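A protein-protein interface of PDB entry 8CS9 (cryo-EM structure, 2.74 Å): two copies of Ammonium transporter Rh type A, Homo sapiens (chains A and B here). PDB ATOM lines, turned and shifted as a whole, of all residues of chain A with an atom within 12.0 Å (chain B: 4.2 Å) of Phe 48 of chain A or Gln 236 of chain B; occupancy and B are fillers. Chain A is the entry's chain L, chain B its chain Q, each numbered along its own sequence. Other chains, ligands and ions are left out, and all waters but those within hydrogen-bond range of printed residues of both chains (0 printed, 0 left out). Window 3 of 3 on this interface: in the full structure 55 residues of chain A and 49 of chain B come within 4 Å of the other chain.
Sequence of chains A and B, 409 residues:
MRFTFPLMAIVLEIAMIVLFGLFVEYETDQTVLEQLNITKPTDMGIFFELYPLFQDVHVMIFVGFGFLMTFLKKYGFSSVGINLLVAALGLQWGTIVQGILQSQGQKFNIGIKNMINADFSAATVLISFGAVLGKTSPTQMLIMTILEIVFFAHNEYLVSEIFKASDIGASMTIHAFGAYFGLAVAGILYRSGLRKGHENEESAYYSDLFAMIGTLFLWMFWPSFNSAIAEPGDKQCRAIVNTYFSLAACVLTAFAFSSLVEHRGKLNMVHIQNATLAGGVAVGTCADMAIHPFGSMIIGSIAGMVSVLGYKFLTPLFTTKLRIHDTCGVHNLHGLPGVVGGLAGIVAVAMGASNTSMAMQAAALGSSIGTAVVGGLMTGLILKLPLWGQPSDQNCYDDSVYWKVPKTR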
ATOM      1  N   TYR A  26      20.465   9.370  22.337  1.00  0.00           N
ATOM      2  CA  TYR A  26      19.684  10.473  21.783  1.00  0.00           C
ATOM      3  C   TYR A  26      18.812  10.002  20.625  1.00  0.00           C
ATOM      4  O   TYR A  26      17.954  10.740  20.141  1.00  0.00           O
ATOM      5  CB  TYR A  26      20.595  11.610  21.314  1.00  0.00           C
ATOM      6  CG  TYR A  26      21.201  12.426  22.428  1.00  0.00           C
ATOM      7  CD1 TYR A  26      20.397  13.157  23.295  1.00  0.00           C
ATOM      8  CD2 TYR A  26      22.576  12.483  22.605  1.00  0.00           C
ATOM      9  CE1 TYR A  26      20.946  13.910  24.311  1.00  0.00           C
ATOM     10  CE2 TYR A  26      23.134  13.235  23.617  1.00  0.00           C
ATOM     11  CZ  TYR A  26      22.315  13.946  24.469  1.00  0.00           C
ATOM     12  OH  TYR A  26      22.867  14.696  25.477  1.00  0.00           O
ATOM     13  N   PHE A  48       9.674  17.546  17.236  1.00  0.00           N
ATOM     14  CA  PHE A  48       9.598  18.896  17.777  1.00  0.00           C
ATOM     15  C   PHE A  48       8.213  19.508  17.596  1.00  0.00           C
ATOM     16  O   PHE A  48       7.943  20.600  18.088  1.00  0.00           O
ATOM     17  CB  PHE A  48      10.644  19.796  17.123  1.00  0.00           C
ATOM     18  CG  PHE A  48      11.039  20.973  17.967  1.00  0.00           C
ATOM     19  CD1 PHE A  48      11.390  20.803  19.294  1.00  0.00           C
ATOM     20  CD2 PHE A  48      11.045  22.250  17.436  1.00  0.00           C
ATOM     21  CE1 PHE A  48      11.748  21.885  20.073  1.00  0.00           C
ATOM     22  CE2 PHE A  48      11.404  23.335  18.212  1.00  0.00           C
ATOM     23  CZ  PHE A  48      11.756  23.150  19.534  1.00  0.00           C
ATOM     24  N   GLU A  49       7.338  18.806  16.877  1.00  0.00           N
ATOM     25  CA  GLU A  49       5.968  19.271  16.707  1.00  0.00           C
ATOM     26  C   GLU A  49       5.080  18.912  17.890  1.00  0.00           C
ATOM     27  O   GLU A  49       3.983  19.465  18.014  1.00  0.00           O
ATOM     28  CB  GLU A  49       5.370  18.697  15.423  1.00  0.00           C
ATOM     29  N   LEU A  50       5.525  18.001  18.752  1.00  0.00           N
ATOM     30  CA  LEU A  50       4.769  17.587  19.923  1.00  0.00           C
ATOM     31  C   LEU A  50       5.267  18.230  21.208  1.00  0.00           C
ATOM     32  O   LEU A  50       4.736  17.930  22.280  1.00  0.00           O
ATOM     33  CB  LEU A  50       4.815  16.062  20.063  1.00  0.00           C
ATOM     34  CG  LEU A  50       4.072  15.216  19.028  1.00  0.00           C
ATOM     35  CD1 LEU A  50       3.686  13.882  19.630  1.00  0.00           C
ATOM     36  CD2 LEU A  50       2.840  15.944  18.506  1.00  0.00           C
ATOM     37  N   TYR A  51       6.279  19.093  21.126  1.00  0.00           N
ATOM     38  CA  TYR A  51       6.816  19.722  22.329  1.00  0.00           C
ATOM     39  C   TYR A  51       5.818  20.610  23.075  1.00  0.00           C
ATOM     40  O   TYR A  51       5.819  20.560  24.317  1.00  0.00           O
ATOM     41  CB  TYR A  51       8.092  20.500  21.983  1.00  0.00           C
ATOM     42  CG  TYR A  51       8.776  21.095  23.190  1.00  0.00           C
ATOM     43  CD1 TYR A  51       9.275  20.282  24.199  1.00  0.00           C
ATOM     44  CD2 TYR A  51       8.923  22.467  23.323  1.00  0.00           C
ATOM     45  CE1 TYR A  51       9.897  20.818  25.304  1.00  0.00           C
ATOM     46  CE2 TYR A  51       9.548  23.012  24.424  1.00  0.00           C
ATOM     47  CZ  TYR A  51      10.032  22.184  25.412  1.00  0.00           C
ATOM     48  OH  TYR A  51      10.654  22.723  26.511  1.00  0.00           O
ATOM     49  N   PRO A  52       4.996  21.456  22.430  1.00  0.00           N
ATOM     50  CA  PRO A  52       3.979  22.188  23.209  1.00  0.00           C
ATOM     51  C   PRO A  52       3.002  21.285  23.948  1.00  0.00           C
ATOM     52  O   PRO A  52       2.630  21.584  25.092  1.00  0.00           O
ATOM     53  CB  PRO A  52       3.272  23.040  22.147  1.00  0.00           C
ATOM     54  CG  PRO A  52       4.269  23.211  21.081  1.00  0.00           C
ATOM     55  CD  PRO A  52       5.038  21.933  21.033  1.00  0.00           C
ATOM     56  N   LEU A  53       2.585  20.177  23.332  1.00  0.00           N
ATOM     57  CA  LEU A  53       1.706  19.239  24.023  1.00  0.00           C
ATOM     58  C   LEU A  53       2.425  18.572  25.187  1.00  0.00           C
ATOM     59  O   LEU A  53       1.829  18.349  26.251  1.00  0.00           O
ATOM     60  CB  LEU A  53       1.174  18.193  23.043  1.00  0.00           C
ATOM     61  CG  LEU A  53       0.487  18.724  21.782  1.00  0.00           C
ATOM     62  CD1 LEU A  53      -0.172  17.589  21.021  1.00  0.00           C
ATOM     63  CD2 LEU A  53      -0.529  19.805  22.116  1.00  0.00           C
ATOM     64  N   PHE A  54       3.712  18.259  25.007  1.00  0.00           N
ATOM     65  CA  PHE A  54       4.502  17.745  26.118  1.00  0.00           C
ATOM     66  C   PHE A  54       4.556  18.748  27.257  1.00  0.00           C
ATOM     67  O   PHE A  54       4.472  18.368  28.426  1.00  0.00           O
ATOM     68  CB  PHE A  54       5.923  17.409  25.678  1.00  0.00           C
ATOM     69  CG  PHE A  54       6.907  17.412  26.816  1.00  0.00           C
ATOM     70  CD1 PHE A  54       6.934  16.367  27.724  1.00  0.00           C
ATOM     71  CD2 PHE A  54       7.776  18.478  27.003  1.00  0.00           C
ATOM     72  CE1 PHE A  54       7.816  16.371  28.781  1.00  0.00           C
ATOM     73  CE2 PHE A  54       8.657  18.487  28.062  1.00  0.00           C
ATOM     74  CZ  PHE A  54       8.678  17.433  28.952  1.00  0.00           C
ATOM     75  N   GLN A  55       4.737  20.029  26.940  1.00  0.00           N
ATOM     76  CA  GLN A  55       4.813  21.031  27.994  1.00  0.00           C
ATOM     77  C   GLN A  55       3.477  21.195  28.706  1.00  0.00           C
ATOM     78  O   GLN A  55       3.451  21.429  29.917  1.00  0.00           O
ATOM     79  CB  GLN A  55       5.292  22.369  27.430  1.00  0.00           C
ATOM     80  CG  GLN A  55       6.811  22.538  27.419  1.00  0.00           C
ATOM     81  CD  GLN A  55       7.457  22.363  28.788  1.00  0.00           C
ATOM     82  OE1 GLN A  55       6.820  22.548  29.824  1.00  0.00           O
ATOM     83  NE2 GLN A  55       8.732  21.997  28.792  1.00  0.00           N
ATOM     84  N   ASP A  56       2.367  21.069  27.979  1.00  0.00           N
ATOM     85  CA  ASP A  56       1.058  21.076  28.628  1.00  0.00           C
ATOM     86  C   ASP A  56       0.914  19.899  29.587  1.00  0.00           C
ATOM     87  O   ASP A  56       0.425  20.052  30.715  1.00  0.00           O
ATOM     88  CB  ASP A  56      -0.048  21.047  27.575  1.00  0.00           C
ATOM     89  CG  ASP A  56      -0.090  22.302  26.737  1.00  0.00           C
ATOM     90  OD1 ASP A  56       0.253  23.384  27.255  1.00  0.00           O
ATOM     91  OD2 ASP A  56      -0.472  22.207  25.553  1.00  0.00           O
ATOM     92  N   ILE A 110      15.704   8.456  22.636  1.00  0.00           N
ATOM     93  CA  ILE A 110      14.777   9.267  23.415  1.00  0.00           C
ATOM     94  C   ILE A 110      14.294  10.422  22.553  1.00  0.00           C
ATOM     95  O   ILE A 110      15.101  11.224  22.068  1.00  0.00           O
ATOM     96  CB  ILE A 110      15.410   9.785  24.715  1.00  0.00           C
ATOM     97  CG1 ILE A 110      15.640   8.624  25.681  1.00  0.00           C
ATOM     98  CG2 ILE A 110      14.543  10.867  25.345  1.00  0.00           C
ATOM     99  CD1 ILE A 110      15.916   9.068  27.085  1.00  0.00           C
ATOM    100  N   GLY A 111      12.981  10.503  22.364  1.00  0.00           N
ATOM    101  CA  GLY A 111      12.373  11.623  21.680  1.00  0.00           C
ATOM    102  C   GLY A 111      11.361  12.320  22.564  1.00  0.00           C
ATOM    103  O   GLY A 111      11.409  12.189  23.790  1.00  0.00           O
ATOM    104  N   ILE A 112      10.441  13.068  21.954  1.00  0.00           N
ATOM    105  CA  ILE A 112       9.414  13.748  22.734  1.00  0.00           C
ATOM    106  C   ILE A 112       8.380  12.753  23.257  1.00  0.00           C
ATOM    107  O   ILE A 112       7.798  12.954  24.333  1.00  0.00           O
ATOM    108  CB  ILE A 112       8.777  14.871  21.891  1.00  0.00           C
ATOM    109  CG1 ILE A 112       7.970  15.818  22.777  1.00  0.00           C
ATOM    110  CG2 ILE A 112       7.938  14.307  20.749  1.00  0.00           C
ATOM    111  CD1 ILE A 112       8.838  16.709  23.632  1.00  0.00           C
ATOM    112  N   LYS A 113       8.153  11.657  22.527  1.00  0.00           N
ATOM    113  CA  LYS A 113       7.141  10.686  22.931  1.00  0.00           C
ATOM    114  C   LYS A 113       7.572   9.923  24.177  1.00  0.00           C
ATOM    115  O   LYS A 113       6.737   9.591  25.028  1.00  0.00           O
ATOM    116  CB  LYS A 113       6.855   9.723  21.781  1.00  0.00           C
ATOM    117  CG  LYS A 113       5.585  10.041  21.020  1.00  0.00           C
ATOM    118  CD  LYS A 113       5.133   8.859  20.185  1.00  0.00           C
ATOM    119  CE  LYS A 113       3.903   9.199  19.360  1.00  0.00           C
ATOM    120  NZ  LYS A 113       4.016  10.540  18.723  1.00  0.00           N
ATOM    121  N   ASN A 114       8.871   9.637  24.299  1.00  0.00           N
ATOM    122  CA  ASN A 114       9.383   8.999  25.506  1.00  0.00           C
ATOM    123  C   ASN A 114       9.156   9.883  26.724  1.00  0.00           C
ATOM    124  O   ASN A 114       8.754   9.400  27.789  1.00  0.00           O
ATOM    125  CB  ASN A 114      10.871   8.692  25.343  1.00  0.00           C
ATOM    126  CG  ASN A 114      11.152   7.765  24.181  1.00  0.00           C
ATOM    127  OD1 ASN A 114      11.191   8.193  23.030  1.00  0.00           O
ATOM    128  ND2 ASN A 114      11.349   6.490  24.477  1.00  0.00           N
ATOM    129  N   MET A 115       9.398  11.185  26.573  1.00  0.00           N
ATOM    130  CA  MET A 115       9.157  12.131  27.657  1.00  0.00           C
ATOM    131  C   MET A 115       7.680  12.187  28.021  1.00  0.00           C
ATOM    132  O   MET A 115       7.323  12.211  29.205  1.00  0.00           O
ATOM    133  CB  MET A 115       9.663  13.510  27.246  1.00  0.00           C
ATOM    134  CG  MET A 115      11.166  13.663  27.338  1.00  0.00           C
ATOM    135  SD  MET A 115      11.817  14.827  26.134  1.00  0.00           S
ATOM    136  CE  MET A 115      11.301  16.367  26.876  1.00  0.00           C
ATOM    137  N   ILE A 116       6.804  12.198  27.013  1.00  0.00           N
ATOM    138  CA  ILE A 116       5.367  12.241  27.273  1.00  0.00           C
ATOM    139  C   ILE A 116       4.924  10.997  28.039  1.00  0.00           C
ATOM    140  O   ILE A 116       4.167  11.085  29.015  1.00  0.00           O
ATOM    141  CB  ILE A 116       4.600  12.412  25.949  1.00  0.00           C
ATOM    142  CG1 ILE A 116       4.824  13.818  25.388  1.00  0.00           C
ATOM    143  CG2 ILE A 116       3.121  12.166  26.145  1.00  0.00           C
ATOM    144  CD1 ILE A 116       4.388  13.992  23.951  1.00  0.00           C
ATOM    145  N   ALA A 228      -1.839  13.953  23.172  1.00  0.00           N
ATOM    146  CA  ALA A 228      -0.399  14.099  22.975  1.00  0.00           C
ATOM    147  C   ALA A 228       0.152  13.005  22.068  1.00  0.00           C
ATOM    148  O   ALA A 228       0.823  13.292  21.070  1.00  0.00           O
ATOM    149  CB  ALA A 228       0.315  14.096  24.326  1.00  0.00           C
ATOM    150  N   PRO A 232      -1.478  11.530  14.415  1.00  0.00           N
ATOM    151  CA  PRO A 232      -1.711  12.844  13.801  1.00  0.00           C
ATOM    152  C   PRO A 232      -2.709  12.760  12.656  1.00  0.00           C
ATOM    153  O   PRO A 232      -2.654  11.856  11.820  1.00  0.00           O
ATOM    154  CB  PRO A 232      -0.322  13.269  13.311  1.00  0.00           C
ATOM    155  CG  PRO A 232       0.526  12.057  13.351  1.00  0.00           C
ATOM    156  CD  PRO A 232      -0.086  11.070  14.283  1.00  0.00           C
ATOM    157  N   GLN A 236      -6.103  12.981  16.416  1.00  0.00           N
ATOM    158  CA  GLN A 236      -5.645  13.995  17.363  1.00  0.00           C
ATOM    159  C   GLN A 236      -6.672  15.113  17.521  1.00  0.00           C
ATOM    160  O   GLN A 236      -6.947  15.564  18.643  1.00  0.00           O
ATOM    161  CB  GLN A 236      -4.298  14.554  16.904  1.00  0.00           C
ATOM    162  CG  GLN A 236      -3.650  15.527  17.867  1.00  0.00           C
ATOM    163  CD  GLN A 236      -2.139  15.518  17.767  1.00  0.00           C
ATOM    164  OE1 GLN A 236      -1.572  15.914  16.750  1.00  0.00           O
ATOM    165  NE2 GLN A 236      -1.478  15.066  18.824  1.00  0.00           N
ATOM    166  N   LEU B  50       9.226  29.128  16.939  1.00  0.00           N
ATOM    167  CA  LEU B  50       9.921  29.486  18.165  1.00  0.00           C
ATOM    168  C   LEU B  50       9.023  30.189  19.172  1.00  0.00           C
ATOM    169  O   LEU B  50       9.433  30.370  20.324  1.00  0.00           O
ATOM    170  CB  LEU B  50      11.119  30.384  17.843  1.00  0.00           C
ATOM    171  CG  LEU B  50      12.408  29.722  17.354  1.00  0.00           C
ATOM    172  CD1 LEU B  50      13.599  30.599  17.683  1.00  0.00           C
ATOM    173  CD2 LEU B  50      12.581  28.334  17.950  1.00  0.00           C
ATOM    174  N   LEU B  53       8.284  28.359  22.602  1.00  0.00           N
ATOM    175  CA  LEU B  53       9.429  28.413  23.501  1.00  0.00           C
ATOM    176  C   LEU B  53       9.571  29.798  24.116  1.00  0.00           C
ATOM    177  O   LEU B  53       9.884  29.927  25.306  1.00  0.00           O
ATOM    178  CB  LEU B  53      10.699  28.006  22.750  1.00  0.00           C
ATOM    179  CG  LEU B  53      11.008  26.506  22.672  1.00  0.00           C
ATOM    180  CD1 LEU B  53      10.021  25.763  21.782  1.00  0.00           C
ATOM    181  CD2 LEU B  53      12.428  26.271  22.188  1.00  0.00           C
ATOM    182  N   SER B 227      16.754  25.800  25.299  1.00  0.00           N
ATOM    183  CA  SER B 227      16.732  25.436  23.889  1.00  0.00           C
ATOM    184  C   SER B 227      16.145  26.501  22.972  1.00  0.00           C
ATOM    185  O   SER B 227      15.986  26.239  21.776  1.00  0.00           O
ATOM    186  CB  SER B 227      15.959  24.126  23.695  1.00  0.00           C
ATOM    187  OG  SER B 227      14.570  24.325  23.877  1.00  0.00           O
ATOM    188  N   ALA B 230      19.045  27.652  20.623  1.00  0.00           N
ATOM    189  CA  ALA B 230      19.779  26.551  20.011  1.00  0.00           C
ATOM    190  C   ALA B 230      19.318  26.285  18.580  1.00  0.00           C
ATOM    191  O   ALA B 230      18.153  26.485  18.228  1.00  0.00           O
ATOM    192  CB  ALA B 230      19.622  25.281  20.845  1.00  0.00           C
ATOM    193  N   GLU B 231      20.260  25.848  17.753  1.00  0.00           N
ATOM    194  CA  GLU B 231      19.987  25.648  16.334  1.00  0.00           C
ATOM    195  C   GLU B 231      18.996  24.507  16.145  1.00  0.00           C
ATOM    196  O   GLU B 231      19.128  23.464  16.796  1.00  0.00           O
ATOM    197  CB  GLU B 231      21.282  25.356  15.580  1.00  0.00           C
ATOM    198  CG  GLU B 231      21.853  26.552  14.832  1.00  0.00           C
ATOM    199  CD  GLU B 231      22.614  27.513  15.731  1.00  0.00           C
ATOM    200  OE1 GLU B 231      22.638  27.300  16.962  1.00  0.00           O
ATOM    201  OE2 GLU B 231      23.192  28.486  15.203  1.00  0.00           O
ATOM    202  N   PRO B 232      17.992  24.668  15.281  1.00  0.00           N
ATOM    203  CA  PRO B 232      16.987  23.613  15.106  1.00  0.00           C
ATOM    204  C   PRO B 232      17.603  22.326  14.582  1.00  0.00           C
ATOM    205  O   PRO B 232      18.567  22.340  13.815  1.00  0.00           O
ATOM    206  CB  PRO B 232      16.006  24.218  14.095  1.00  0.00           C
ATOM    207  CG  PRO B 232      16.243  25.682  14.136  1.00  0.00           C
ATOM    208  CD  PRO B 232      17.666  25.890  14.530  1.00  0.00           C
ATOM    209  N   GLY B 233      17.030  21.205  15.009  1.00  0.00           N
ATOM    210  CA  GLY B 233      17.559  19.905  14.657  1.00  0.00           C
ATOM    211  C   GLY B 233      17.973  19.104  15.871  1.00  0.00           C
ATOM    212  O   GLY B 233      17.210  18.982  16.832  1.00  0.00           O
ATOM    213  N   ASP B 234      19.183  18.548  15.840  1.00  0.00           N
ATOM    214  CA  ASP B 234      19.655  17.740  16.956  1.00  0.00           C
ATOM    215  C   ASP B 234      20.073  18.587  18.151  1.00  0.00           C
ATOM    216  O   ASP B 234      20.003  18.114  19.287  1.00  0.00           O
ATOM    217  CB  ASP B 234      20.818  16.854  16.509  1.00  0.00           C
ATOM    218  CG  ASP B 234      20.551  16.171  15.184  1.00  0.00           C
ATOM    219  OD1 ASP B 234      19.406  16.250  14.694  1.00  0.00           O
ATOM    220  OD2 ASP B 234      21.485  15.551  14.634  1.00  0.00           O
ATOM    221  N   LYS B 235      20.504  19.829  17.921  1.00  0.00           N
ATOM    222  CA  LYS B 235      20.983  20.659  19.023  1.00  0.00           C
ATOM    223  C   LYS B 235      19.845  21.067  19.953  1.00  0.00           C
ATOM    224  O   LYS B 235      19.975  20.977  21.179  1.00  0.00           O
ATOM    225  CB  LYS B 235      21.700  21.890  18.473  1.00  0.00           C
ATOM    226  CG  LYS B 235      23.063  21.587  17.866  1.00  0.00           C
ATOM    227  CD  LYS B 235      24.195  22.030  18.773  1.00  0.00           C
ATOM    228  CE  LYS B 235      25.470  22.279  17.984  1.00  0.00           C
ATOM    229  NZ  LYS B 235      25.211  23.051  16.741  1.00  0.00           N
ATOM    230  N   GLN B 236      18.719  21.506  19.385  1.00  0.00           N
ATOM    231  CA  GLN B 236      17.564  21.884  20.194  1.00  0.00           C
ATOM    232  C   GLN B 236      17.011  20.692  20.966  1.00  0.00           C
ATOM    233  O   GLN B 236      16.685  20.806  22.157  1.00  0.00           O
ATOM    234  CB  GLN B 236      16.488  22.489  19.295  1.00  0.00           C
ATOM    235  CG  GLN B 236      15.814  23.714  19.864  1.00  0.00           C
ATOM    236  CD  GLN B 236      14.902  24.396  18.870  1.00  0.00           C
ATOM    237  OE1 GLN B 236      14.709  23.914  17.755  1.00  0.00           O
ATOM    238  NE2 GLN B 236      14.339  25.530  19.265  1.00  0.00           N
ATOM    239  N   CYS B 237      16.905  19.537  20.303  1.00  0.00           N
ATOM    240  CA  CYS B 237      16.412  18.336  20.966  1.00  0.00           C
ATOM    241  C   CYS B 237      17.351  17.897  22.082  1.00  0.00           C
ATOM    242  O   CYS B 237      16.897  17.491  23.160  1.00  0.00           O
ATOM    243  CB  CYS B 237      16.225  17.216  19.944  1.00  0.00           C
ATOM    244  SG  CYS B 237      15.827  15.607  20.658  1.00  0.00           S
ATOM    245  N   ARG B 238      18.663  17.967  21.841  1.00  0.00           N
ATOM    246  CA  ARG B 238      19.625  17.616  22.879  1.00  0.00           C
ATOM    247  C   ARG B 238      19.520  18.561  24.066  1.00  0.00           C
ATOM    248  O   ARG B 238      19.584  18.124  25.219  1.00  0.00           O
ATOM    249  CB  ARG B 238      21.047  17.616  22.316  1.00  0.00           C
ATOM    250  CG  ARG B 238      21.427  16.346  21.578  1.00  0.00           C
ATOM    251  CD  ARG B 238      22.935  16.163  21.531  1.00  0.00           C
ATOM    252  NE  ARG B 238      23.622  17.296  20.925  1.00  0.00           N
ATOM    253  CZ  ARG B 238      23.960  17.372  19.645  1.00  0.00           C
ATOM    254  NH1 ARG B 238      23.679  16.396  18.797  1.00  0.00           N
ATOM    255  NH2 ARG B 238      24.599  18.451  19.205  1.00  0.00           N
ATOM    256  N   ALA B 239      19.350  19.859  23.805  1.00  0.00           N
ATOM    257  CA  ALA B 239      19.185  20.816  24.895  1.00  0.00           C
ATOM    258  C   ALA B 239      17.945  20.504  25.721  1.00  0.00           C
ATOM    259  O   ALA B 239      17.999  20.500  26.958  1.00  0.00           O
ATOM    260  CB  ALA B 239      19.122  22.238  24.340  1.00  0.00           C
ATOM    261  N   ILE B 240      16.830  20.198  25.053  1.00  0.00           N
ATOM    262  CA  ILE B 240      15.584  19.917  25.766  1.00  0.00           C
ATOM    263  C   ILE B 240      15.720  18.656  26.615  1.00  0.00           C
ATOM    264  O   ILE B 240      15.377  18.647  27.805  1.00  0.00           O
ATOM    265  CB  ILE B 240      14.413  19.815  24.772  1.00  0.00           C
ATOM    266  CG1 ILE B 240      13.866  21.206  24.461  1.00  0.00           C
ATOM    267  CG2 ILE B 240      13.304  18.946  25.319  1.00  0.00           C
ATOM    268  CD1 ILE B 240      12.969  21.250  23.265  1.00  0.00           C
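4 positions are printed for both chains. Of the 7 pairs that touch across the chains among the printed residues, none has its exchanged pair printed and touching as well.
Phe 48 of chain A touches three residues of chain B. Leu 50 of chain B touches none of the printed residues of chain A. No residue of chain A comes within 4 Å of Ala 230 of chain B. No residue of chain A comes within 4 Å of Pro 232 of chain B. No residue of chain A comes within 4 Å of Gly 233 of chain B. No residue of chain A comes within 4 Å of Lys 235 of chain B. No residue of chain A comes within 4 Å of Cys 237 of chain B. No residue of chain A comes within 4 Å of Ala 239 of chain B. Ile 240 of chain B touches three residues of chain A. Of the printed residues of chain B, Tyr 51 of chain A touches Leu 53 (3.8 Å) and Ile 240 (3.7 Å). Printed residues of chain B within 4 Å of Met 115 of chain A: Ile 240. Ile 110 of chain A touches none of the printed residues of chain B. The nearest residue of chain A that does not touch Gln 236 of chain B is Tyr 51 of chain A (7.4 Å). The nearest printed residue of chain B that does not touch Met 115 of chain A is Cys 237 of chain B (6.5 Å).
NE2 of Gln 55 of chain A is in hydrogen-bond range of OH of Tyr 51 of chain A (3.1 Å). The backbone carbonyl oxygen (O) of Ser 227 of chain B is in hydrogen-bond range of the side-chain amide nitrogen (NE2) of Gln 236 of chain B (3.1 Å). The backbone carbonyl oxygen (O) of Glu 231 of chain B is in hydrogen-bond range of the backbone NH (N) of Gln 236 of chain B (3.3 Å).
Hydrophobic or aromatic side chains of chain B within 4 Å of the printed part of chain A: Leu 53 and Ile 240. Among the printed residues, no Asp or Glu carboxylate lies within 4 Å of a Lys or Arg side-chain nitrogen of the other chain.
Among the printed residues, pairs that only touch across the chains: Phe 48 of chain A with Gln 236 of chain B, Phe 48 of chain A with Ile 240 of chain B, Tyr 26 of chain A with Arg 238 of chain B, Met 115 of chain A with Ile 240 of chain B, Tyr 51 of chain A with Ile 240 of chain B, Tyr 51 of chain A with Leu 53 of chain B and Phe 48 of chain A with Leu 53 of chain B.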
